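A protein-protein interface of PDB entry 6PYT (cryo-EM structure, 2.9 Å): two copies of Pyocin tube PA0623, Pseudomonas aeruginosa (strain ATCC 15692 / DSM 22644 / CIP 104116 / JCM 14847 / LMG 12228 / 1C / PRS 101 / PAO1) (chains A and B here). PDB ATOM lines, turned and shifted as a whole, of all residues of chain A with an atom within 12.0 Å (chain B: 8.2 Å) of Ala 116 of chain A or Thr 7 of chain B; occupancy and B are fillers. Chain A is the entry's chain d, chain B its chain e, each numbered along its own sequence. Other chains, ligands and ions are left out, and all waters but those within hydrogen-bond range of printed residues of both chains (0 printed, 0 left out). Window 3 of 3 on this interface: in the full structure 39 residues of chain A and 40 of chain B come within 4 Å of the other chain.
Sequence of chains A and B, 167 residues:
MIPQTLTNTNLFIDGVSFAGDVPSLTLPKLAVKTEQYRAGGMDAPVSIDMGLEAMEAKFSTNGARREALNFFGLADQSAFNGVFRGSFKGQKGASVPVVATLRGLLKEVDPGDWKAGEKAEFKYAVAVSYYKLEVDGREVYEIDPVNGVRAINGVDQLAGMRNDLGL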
ATOM      1  N   ASN A  62      19.520  16.071  -4.248  1.00  0.00           N
ATOM      2  CA  ASN A  62      19.557  15.448  -5.560  1.00  0.00           C
ATOM      3  C   ASN A  62      20.929  14.908  -5.929  1.00  0.00           C
ATOM      4  O   ASN A  62      21.163  14.598  -7.100  1.00  0.00           O
ATOM      5  CB  ASN A  62      19.012  16.404  -6.629  1.00  0.00           C
ATOM      6  CG  ASN A  62      19.669  17.736  -6.625  1.00  0.00           C
ATOM      7  OD1 ASN A  62      20.665  17.961  -5.954  1.00  0.00           O
ATOM      8  ND2 ASN A  62      19.081  18.658  -7.359  1.00  0.00           N
ATOM      9  N   GLY A  63      21.826  14.778  -4.960  1.00  0.00           N
ATOM     10  CA  GLY A  63      22.950  13.880  -5.039  1.00  0.00           C
ATOM     11  C   GLY A  63      22.683  12.620  -4.245  1.00  0.00           C
ATOM     12  O   GLY A  63      21.546  12.319  -3.870  1.00  0.00           O
ATOM     13  N   ALA A  64      23.750  11.870  -3.977  1.00  0.00           N
ATOM     14  CA  ALA A  64      23.597  10.618  -3.243  1.00  0.00           C
ATOM     15  C   ALA A  64      23.362  10.875  -1.763  1.00  0.00           C
ATOM     16  O   ALA A  64      22.292  10.557  -1.235  1.00  0.00           O
ATOM     17  CB  ALA A  64      24.827   9.743  -3.454  1.00  0.00           C
ATOM     18  N   GLY A 112      12.897   9.422  -6.680  1.00  0.00           N
ATOM     19  CA  GLY A 112      11.883   9.522  -7.710  1.00  0.00           C
ATOM     20  C   GLY A 112      12.206   8.696  -8.934  1.00  0.00           C
ATOM     21  O   GLY A 112      12.888   7.669  -8.867  1.00  0.00           O
ATOM     22  N   ASP A 113      11.697   9.145 -10.072  1.00  0.00           N
ATOM     23  CA  ASP A 113      12.027   8.494 -11.325  1.00  0.00           C
ATOM     24  C   ASP A 113      13.472   8.792 -11.693  1.00  0.00           C
ATOM     25  O   ASP A 113      13.971   9.895 -11.471  1.00  0.00           O
ATOM     26  CB  ASP A 113      11.084   8.961 -12.427  1.00  0.00           C
ATOM     27  N   TRP A 114      14.158   7.787 -12.213  1.00  0.00           N
ATOM     28  CA  TRP A 114      15.523   7.941 -12.694  1.00  0.00           C
ATOM     29  C   TRP A 114      15.512   7.832 -14.211  1.00  0.00           C
ATOM     30  O   TRP A 114      15.686   6.754 -14.774  1.00  0.00           O
ATOM     31  CB  TRP A 114      16.455   6.916 -12.099  1.00  0.00           C
ATOM     32  CG  TRP A 114      16.874   7.168 -10.717  1.00  0.00           C
ATOM     33  CD1 TRP A 114      16.471   8.174  -9.911  1.00  0.00           C
ATOM     34  CD2 TRP A 114      17.865   6.442  -9.993  1.00  0.00           C
ATOM     35  NE1 TRP A 114      17.116   8.098  -8.704  1.00  0.00           N
ATOM     36  CE2 TRP A 114      17.989   7.045  -8.737  1.00  0.00           C
ATOM     37  CE3 TRP A 114      18.662   5.339 -10.292  1.00  0.00           C
ATOM     38  CZ2 TRP A 114      18.864   6.574  -7.771  1.00  0.00           C
ATOM     39  CZ3 TRP A 114      19.526   4.873  -9.335  1.00  0.00           C
ATOM     40  CH2 TRP A 114      19.621   5.488  -8.092  1.00  0.00           C
ATOM     41  N   LYS A 115      15.306   8.956 -14.868  1.00  0.00           N
ATOM     42  CA  LYS A 115      15.553   9.036 -16.291  1.00  0.00           C
ATOM     43  C   LYS A 115      16.988   9.482 -16.515  1.00  0.00           C
ATOM     44  O   LYS A 115      17.613  10.071 -15.636  1.00  0.00           O
ATOM     45  CB  LYS A 115      14.569   9.994 -16.946  1.00  0.00           C
ATOM     46  CG  LYS A 115      13.140   9.506 -16.880  1.00  0.00           C
ATOM     47  CD  LYS A 115      12.214  10.429 -17.637  1.00  0.00           C
ATOM     48  CE  LYS A 115      10.769   9.995 -17.505  1.00  0.00           C
ATOM     49  NZ  LYS A 115      10.496   8.713 -18.209  1.00  0.00           N
ATOM     50  N   ALA A 116      17.508   9.185 -17.706  1.00  0.00           N
ATOM     51  CA  ALA A 116      18.937   9.345 -17.959  1.00  0.00           C
ATOM     52  C   ALA A 116      19.342  10.814 -17.995  1.00  0.00           C
ATOM     53  O   ALA A 116      20.121  11.275 -17.158  1.00  0.00           O
ATOM     54  CB  ALA A 116      19.315   8.649 -19.263  1.00  0.00           C
ATOM     55  N   GLY A 117      18.795  11.575 -18.923  1.00  0.00           N
ATOM     56  CA  GLY A 117      19.205  12.957 -18.982  1.00  0.00           C
ATOM     57  C   GLY A 117      18.591  13.878 -17.959  1.00  0.00           C
ATOM     58  O   GLY A 117      18.964  15.050 -17.908  1.00  0.00           O
ATOM     59  N   GLU A 118      17.667  13.394 -17.136  1.00  0.00           N
ATOM     60  CA  GLU A 118      16.909  14.235 -16.225  1.00  0.00           C
ATOM     61  C   GLU A 118      17.525  14.194 -14.832  1.00  0.00           C
ATOM     62  O   GLU A 118      18.048  13.164 -14.403  1.00  0.00           O
ATOM     63  CB  GLU A 118      15.439  13.792 -16.188  1.00  0.00           C
ATOM     64  N   LYS A 119      17.491  15.338 -14.153  1.00  0.00           N
ATOM     65  CA  LYS A 119      17.943  15.454 -12.770  1.00  0.00           C
ATOM     66  C   LYS A 119      17.102  14.593 -11.835  1.00  0.00           C
ATOM     67  O   LYS A 119      15.874  14.690 -11.820  1.00  0.00           O
ATOM     68  CB  LYS A 119      17.863  16.918 -12.349  1.00  0.00           C
ATOM     69  CG  LYS A 119      18.337  17.220 -10.960  1.00  0.00           C
ATOM     70  CD  LYS A 119      18.062  18.673 -10.632  1.00  0.00           C
ATOM     71  CE  LYS A 119      19.010  19.586 -11.366  1.00  0.00           C
ATOM     72  NZ  LYS A 119      18.812  21.010 -11.022  1.00  0.00           N
ATOM     73  N   ALA A 120      17.771  13.761 -11.042  1.00  0.00           N
ATOM     74  CA  ALA A 120      17.112  12.842 -10.123  1.00  0.00           C
ATOM     75  C   ALA A 120      17.140  13.408  -8.715  1.00  0.00           C
ATOM     76  O   ALA A 120      18.209  13.731  -8.203  1.00  0.00           O
ATOM     77  CB  ALA A 120      17.789  11.476 -10.140  1.00  0.00           C
ATOM     78  N   GLU A 121      15.977  13.468  -8.076  1.00  0.00           N
ATOM     79  CA  GLU A 121      15.779  14.194  -6.826  1.00  0.00           C
ATOM     80  C   GLU A 121      15.294  13.236  -5.746  1.00  0.00           C
ATOM     81  O   GLU A 121      14.196  12.686  -5.850  1.00  0.00           O
ATOM     82  CB  GLU A 121      14.775  15.323  -7.044  1.00  0.00           C
ATOM     83  N   PHE A 122      16.106  13.040  -4.712  1.00  0.00           N
ATOM     84  CA  PHE A 122      15.693  12.290  -3.530  1.00  0.00           C
ATOM     85  C   PHE A 122      14.816  13.189  -2.671  1.00  0.00           C
ATOM     86  O   PHE A 122      15.293  14.190  -2.141  1.00  0.00           O
ATOM     87  CB  PHE A 122      16.898  11.836  -2.716  1.00  0.00           C
ATOM     88  CG  PHE A 122      17.729  10.770  -3.358  1.00  0.00           C
ATOM     89  CD1 PHE A 122      17.268  10.035  -4.428  1.00  0.00           C
ATOM     90  CD2 PHE A 122      18.984  10.489  -2.862  1.00  0.00           C
ATOM     91  CE1 PHE A 122      18.056   9.054  -4.999  1.00  0.00           C
ATOM     92  CE2 PHE A 122      19.764   9.508  -3.424  1.00  0.00           C
ATOM     93  CZ  PHE A 122      19.299   8.790  -4.488  1.00  0.00           C
ATOM     94  N   GLN B   4      26.076  17.452  -7.064  1.00  0.00           N
ATOM     95  CA  GLN B   4      26.102  16.080  -7.545  1.00  0.00           C
ATOM     96  C   GLN B   4      24.719  15.718  -8.054  1.00  0.00           C
ATOM     97  O   GLN B   4      23.718  16.079  -7.432  1.00  0.00           O
ATOM     98  CB  GLN B   4      26.518  15.140  -6.419  1.00  0.00           C
ATOM     99  CG  GLN B   4      26.630  13.701  -6.786  1.00  0.00           C
ATOM    100  CD  GLN B   4      27.009  12.862  -5.603  1.00  0.00           C
ATOM    101  OE1 GLN B   4      27.114  13.358  -4.491  1.00  0.00           O
ATOM    102  NE2 GLN B   4      27.230  11.582  -5.834  1.00  0.00           N
ATOM    103  N   THR B   5      24.660  15.029  -9.188  1.00  0.00           N
ATOM    104  CA  THR B   5      23.404  14.713  -9.849  1.00  0.00           C
ATOM    105  C   THR B   5      23.604  13.422 -10.630  1.00  0.00           C
ATOM    106  O   THR B   5      24.697  13.154 -11.128  1.00  0.00           O
ATOM    107  CB  THR B   5      22.958  15.870 -10.774  1.00  0.00           C
ATOM    108  OG1 THR B   5      22.829  17.078 -10.016  1.00  0.00           O
ATOM    109  CG2 THR B   5      21.617  15.610 -11.421  1.00  0.00           C
ATOM    110  N   LEU B   6      22.557  12.593 -10.675  1.00  0.00           N
ATOM    111  CA  LEU B   6      22.506  11.448 -11.577  1.00  0.00           C
ATOM    112  C   LEU B   6      22.693  11.902 -13.013  1.00  0.00           C
ATOM    113  O   LEU B   6      22.174  12.943 -13.412  1.00  0.00           O
ATOM    114  CB  LEU B   6      21.179  10.705 -11.430  1.00  0.00           C
ATOM    115  CG  LEU B   6      20.926   9.456 -12.286  1.00  0.00           C
ATOM    116  CD1 LEU B   6      20.207   8.461 -11.510  1.00  0.00           C
ATOM    117  CD2 LEU B   6      20.067   9.752 -13.493  1.00  0.00           C
ATOM    118  N   THR B   7      23.430  11.115 -13.791  1.00  0.00           N
ATOM    119  CA  THR B   7      23.492  11.315 -15.227  1.00  0.00           C
ATOM    120  C   THR B   7      23.107  10.090 -16.032  1.00  0.00           C
ATOM    121  O   THR B   7      22.711  10.241 -17.187  1.00  0.00           O
ATOM    122  CB  THR B   7      24.892  11.750 -15.655  1.00  0.00           C
ATOM    123  OG1 THR B   7      25.865  10.867 -15.085  1.00  0.00           O
ATOM    124  CG2 THR B   7      25.149  13.150 -15.231  1.00  0.00           C
ATOM    125  N   ASN B   8      23.232   8.889 -15.474  1.00  0.00           N
ATOM    126  CA  ASN B   8      23.049   7.675 -16.254  1.00  0.00           C
ATOM    127  C   ASN B   8      22.512   6.576 -15.360  1.00  0.00           C
ATOM    128  O   ASN B   8      22.822   6.517 -14.171  1.00  0.00           O
ATOM    129  CB  ASN B   8      24.362   7.234 -16.902  1.00  0.00           C
ATOM    130  CG  ASN B   8      24.751   8.102 -18.068  1.00  0.00           C
ATOM    131  OD1 ASN B   8      23.954   8.326 -18.974  1.00  0.00           O
ATOM    132  ND2 ASN B   8      25.943   8.672 -18.009  1.00  0.00           N
ATOM    133  N   THR B   9      21.698   5.706 -15.948  1.00  0.00           N
ATOM    134  CA  THR B   9      21.077   4.591 -15.253  1.00  0.00           C
ATOM    135  C   THR B   9      21.368   3.302 -16.006  1.00  0.00           C
ATOM    136  O   THR B   9      21.768   3.321 -17.167  1.00  0.00           O
ATOM    137  CB  THR B   9      19.563   4.788 -15.118  1.00  0.00           C
ATOM    138  OG1 THR B   9      18.986   4.953 -16.417  1.00  0.00           O
ATOM    139  CG2 THR B   9      19.245   6.002 -14.292  1.00  0.00           C
ATOM    140  N   ASN B  10      21.166   2.174 -15.332  1.00  0.00           N
ATOM    141  CA  ASN B  10      21.262   0.874 -15.981  1.00  0.00           C
ATOM    142  C   ASN B  10      20.393  -0.103 -15.204  1.00  0.00           C
ATOM    143  O   ASN B  10      19.964   0.171 -14.087  1.00  0.00           O
ATOM    144  CB  ASN B  10      22.708   0.377 -16.056  1.00  0.00           C
ATOM    145  CG  ASN B  10      22.906  -0.660 -17.131  1.00  0.00           C
ATOM    146  OD1 ASN B  10      22.001  -0.931 -17.905  1.00  0.00           O
ATOM    147  ND2 ASN B  10      24.069  -1.275 -17.156  1.00  0.00           N
ATOM    148  N   VAL B  22      16.091   0.872 -21.220  1.00  0.00           N
ATOM    149  CA  VAL B  22      15.312   1.268 -20.042  1.00  0.00           C
ATOM    150  C   VAL B  22      15.331   2.785 -19.880  1.00  0.00           C
ATOM    151  O   VAL B  22      16.290   3.356 -19.349  1.00  0.00           O
ATOM    152  CB  VAL B  22      15.768   0.526 -18.773  1.00  0.00           C
ATOM    153  CG1 VAL B  22      15.206  -0.858 -18.774  1.00  0.00           C
ATOM    154  CG2 VAL B  22      17.281   0.401 -18.711  1.00  0.00           C
ATOM    155  N   PRO B  23      14.290   3.484 -20.336  1.00  0.00           N
ATOM    156  CA  PRO B  23      14.296   4.947 -20.214  1.00  0.00           C
ATOM    157  C   PRO B  23      14.095   5.459 -18.799  1.00  0.00           C
ATOM    158  O   PRO B  23      14.615   6.532 -18.477  1.00  0.00           O
ATOM    159  CB  PRO B  23      13.149   5.372 -21.137  1.00  0.00           C
ATOM    160  CG  PRO B  23      12.273   4.202 -21.212  1.00  0.00           C
ATOM    161  CD  PRO B  23      13.169   3.013 -21.160  1.00  0.00           C
ATOM    162  N   SER B  24      13.371   4.747 -17.940  1.00  0.00           N
ATOM    163  CA  SER B  24      13.144   5.225 -16.584  1.00  0.00           C
ATOM    164  C   SER B  24      13.219   4.087 -15.579  1.00  0.00           C
ATOM    165  O   SER B  24      12.729   2.987 -15.832  1.00  0.00           O
ATOM    166  CB  SER B  24      11.789   5.921 -16.461  1.00  0.00           C
ATOM    167  OG  SER B  24      10.732   5.005 -16.671  1.00  0.00           O
ATOM    168  N   LEU B  25      13.840   4.367 -14.439  1.00  0.00           N
ATOM    169  CA  LEU B  25      13.879   3.479 -13.290  1.00  0.00           C
ATOM    170  C   LEU B  25      13.149   4.156 -12.143  1.00  0.00           C
ATOM    171  O   LEU B  25      12.948   5.370 -12.148  1.00  0.00           O
ATOM    172  CB  LEU B  25      15.315   3.166 -12.845  1.00  0.00           C
ATOM    173  CG  LEU B  25      16.176   2.107 -13.528  1.00  0.00           C
ATOM    174  CD1 LEU B  25      15.471   0.773 -13.518  1.00  0.00           C
ATOM    175  CD2 LEU B  25      16.593   2.497 -14.930  1.00  0.00           C
ATOM    176  N   GLY B  86      22.766   3.411 -10.853  1.00  0.00           N
ATOM    177  CA  GLY B  86      22.808   4.804 -11.242  1.00  0.00           C
ATOM    178  C   GLY B  86      24.201   5.347 -11.033  1.00  0.00           C
ATOM    179  O   GLY B  86      24.934   4.906 -10.151  1.00  0.00           O
ATOM    180  N   SER B  87      24.565   6.302 -11.870  1.00  0.00           N
ATOM    181  CA  SER B  87      25.854   6.972 -11.782  1.00  0.00           C
ATOM    182  C   SER B  87      25.587   8.431 -11.459  1.00  0.00           C
ATOM    183  O   SER B  87      25.041   9.159 -12.291  1.00  0.00           O
ATOM    184  CB  SER B  87      26.632   6.829 -13.084  1.00  0.00           C
ATOM    185  OG  SER B  87      27.847   7.541 -13.020  1.00  0.00           O
ATOM    186  N   PHE B  88      25.954   8.860 -10.259  1.00  0.00           N
ATOM    187  CA  PHE B  88      25.772  10.250  -9.869  1.00  0.00           C
ATOM    188  C   PHE B  88      27.082  10.973 -10.136  1.00  0.00           C
ATOM    189  O   PHE B  88      28.138  10.521  -9.695  1.00  0.00           O
ATOM    190  CB  PHE B  88      25.375  10.435  -8.400  1.00  0.00           C
ATOM    191  CG  PHE B  88      23.984   9.953  -8.031  1.00  0.00           C
ATOM    192  CD1 PHE B  88      23.209   9.164  -8.855  1.00  0.00           C
ATOM    193  CD2 PHE B  88      23.411  10.420  -6.878  1.00  0.00           C
ATOM    194  CE1 PHE B  88      21.954   8.768  -8.479  1.00  0.00           C
ATOM    195  CE2 PHE B  88      22.138  10.046  -6.517  1.00  0.00           C
ATOM    196  CZ  PHE B  88      21.413   9.222  -7.325  1.00  0.00           C
ATOM    197  N   LYS B  89      27.011  12.094 -10.848  1.00  0.00           N
ATOM    198  CA  LYS B  89      28.197  12.625 -11.510  1.00  0.00           C
ATOM    199  C   LYS B  89      29.063  13.467 -10.583  1.00  0.00           C
ATOM    200  O   LYS B  89      30.215  13.118 -10.313  1.00  0.00           O
ATOM    201  CB  LYS B  89      27.781  13.440 -12.730  1.00  0.00           C
ATOM    202  CG  LYS B  89      28.929  14.005 -13.532  1.00  0.00           C
ATOM    203  CD  LYS B  89      29.756  12.910 -14.158  1.00  0.00           C
ATOM    204  CE  LYS B  89      30.888  13.490 -14.962  1.00  0.00           C
ATOM    205  NZ  LYS B  89      30.362  14.217 -16.139  1.00  0.00           N
ATOM    206  N   GLY B  90      28.543  14.580 -10.104  1.00  0.00           N
ATOM    207  CA  GLY B  90      29.414  15.477  -9.356  1.00  0.00           C
ATOM    208  C   GLY B  90      30.148  16.449 -10.256  1.00  0.00           C
ATOM    209  O   GLY B  90      30.497  16.150 -11.395  1.00  0.00           O
ATOM    210  N   SER B  95      32.491  10.319 -10.223  1.00  0.00           N
ATOM    211  CA  SER B  95      31.219   9.627 -10.371  1.00  0.00           C
ATOM    212  C   SER B  95      31.025   8.602  -9.261  1.00  0.00           C
ATOM    213  O   SER B  95      31.879   7.739  -9.042  1.00  0.00           O
ATOM    214  CB  SER B  95      31.148   8.953 -11.733  1.00  0.00           C
ATOM    215  OG  SER B  95      32.156   7.969 -11.838  1.00  0.00           O
ATOM    216  N   VAL B  96      29.897   8.694  -8.572  1.00  0.00           N
ATOM    217  CA  VAL B  96      29.570   7.867  -7.415  1.00  0.00           C
ATOM    218  C   VAL B  96      28.485   6.879  -7.830  1.00  0.00           C
ATOM    219  O   VAL B  96      27.403   7.305  -8.248  1.00  0.00           O
ATOM    220  CB  VAL B  96      29.104   8.725  -6.230  1.00  0.00           C
ATOM    221  CG1 VAL B  96      28.634   7.856  -5.101  1.00  0.00           C
ATOM    222  CG2 VAL B  96      30.225   9.618  -5.763  1.00  0.00           C
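Of the 14 printed residues of chain A, 10 touch a printed residue of chain B. Printed residues of chain A that touch a printed residue of chain B: Asn 62, Gly 63, Ala 64, Asp 113, Trp 114, Lys 115, Ala 116, Lys 119, Ala 120 and Phe 122. Hydrophobic or aromatic side chains of chain A that line the printed part of chain B: Ala 64, Trp 114, Ala 120 and Phe 122. Hydrophobic or aromatic side chains of chain B that line the printed part of chain A: Leu 6, Leu 25 and Phe 88. Among the printed residues, no Asp or Glu carboxylate lies within 4 Å of a Lys or Arg side-chain nitrogen of the other chain.
No position is printed for both chains. Of the 22 pairs that touch across the chains among the printed residues, none has its exchanged pair printed and touching as well.
Of the printed residues of chain B, Ala 116 of chain A touches Leu 6 and Thr 7. Of chain A, only Ala 116 (2.8 Å) comes within 4 Å of Thr 7 of chain B. No residue of chain B comes within 4 Å of Gly 117 of chain A. Of the printed residues of chain A, Thr 5 of chain B touches Asn 62 (3.5 Å) and Lys 119 (3.7 Å). Of the printed residues of chain A, Thr 9 of chain B touches Trp 114. Ser 87 of chain B touches none of the printed residues of chain A. Of chain A, only Gly 63 (3.5 Å), Ala 64 (3.3 Å), Trp 114 (3.7 Å) and Phe 122 (3.6 Å) come within 4 Å of Phe 88 of chain B. No residue of chain A comes within 4 Å of Lys 89 of chain B. No residue of chain A comes within 4 Å of Gly 90 of chain B. Of the printed residues of chain A, Pro 23 of chain B touches Trp 114 (3.9 Å) and Lys 115 (3.5 Å). Of the printed residues of chain B, Gly 63 of chain A touches Gln 4 and Phe 88. Of the printed residues of chain B, Asp 113 of chain A touches Leu 25 (3.4 Å). Printed residues of chain B within 4 Å of Ala 120 of chain A: Leu 6. Ser 95 of chain B touches none of the printed residues of chain A. Asn 10 of chain B touches none of the printed residues of chain A. The nearest printed residue of chain B that does not touch Ala 116 of chain A is Pro 23 of chain B (4.0003 Å).
C of Gly 63 of chain A touches CE2 of Phe 88 of chain B, at 3.5 Å. CG2 of Thr 9 of chain B touches CB of Trp 114 of chain A, at 3.7 Å. O of Trp 114 of chain A touches O of Pro 23 of chain B, 3.9 Å away. O of Trp 114 of chain A touches CA of Ser 24 of chain B, at 3.5 Å. Phe 88 of chain B touches Trp 114 of chain A (CZ to CZ2, 3.7 Å). Lys 115 of chain A touches Leu 6 of chain B. Lys 115 of chain A touches Pro 23 of chain B. Ala 116 of chain A touches Leu 6 of chain B (O to CD2, 3.97 Å). Lys 119 of chain A touches Thr 5 of chain B. Ala 120 of chain A touches Leu 6 of chain B.
The backbone NH (N) of Gly 63 of chain A lies close to the backbone carbonyl oxygen (O) of Gln 4 of chain B, at 3.4 Å. N of Trp 114 of chain A lies within hydrogen-bond range of O of Leu 25 of chain B (2.7 Å). O of Asn 62 of chain A lies close to O of Gln 4 of chain B, 3.0 Å away. O of Ala 116 of chain A sits close to O of Thr 7 of chain B, 2.8 Å away.
The backbone carbonyl oxygen of Thr 5 of chain B is in hydrogen-bond range of the backbone NH of Lys 89 of chain B, at 2.6 Å. N of Thr 7 of chain B lies within hydrogen-bond range of O of Ser 87 of chain B, at 2.9 Å. The backbone carbonyl oxygen (O) of Phe 88 of chain B is in hydrogen-bond range of the backbone NH (N) of Val 96 of chain B, at 2.8 Å.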
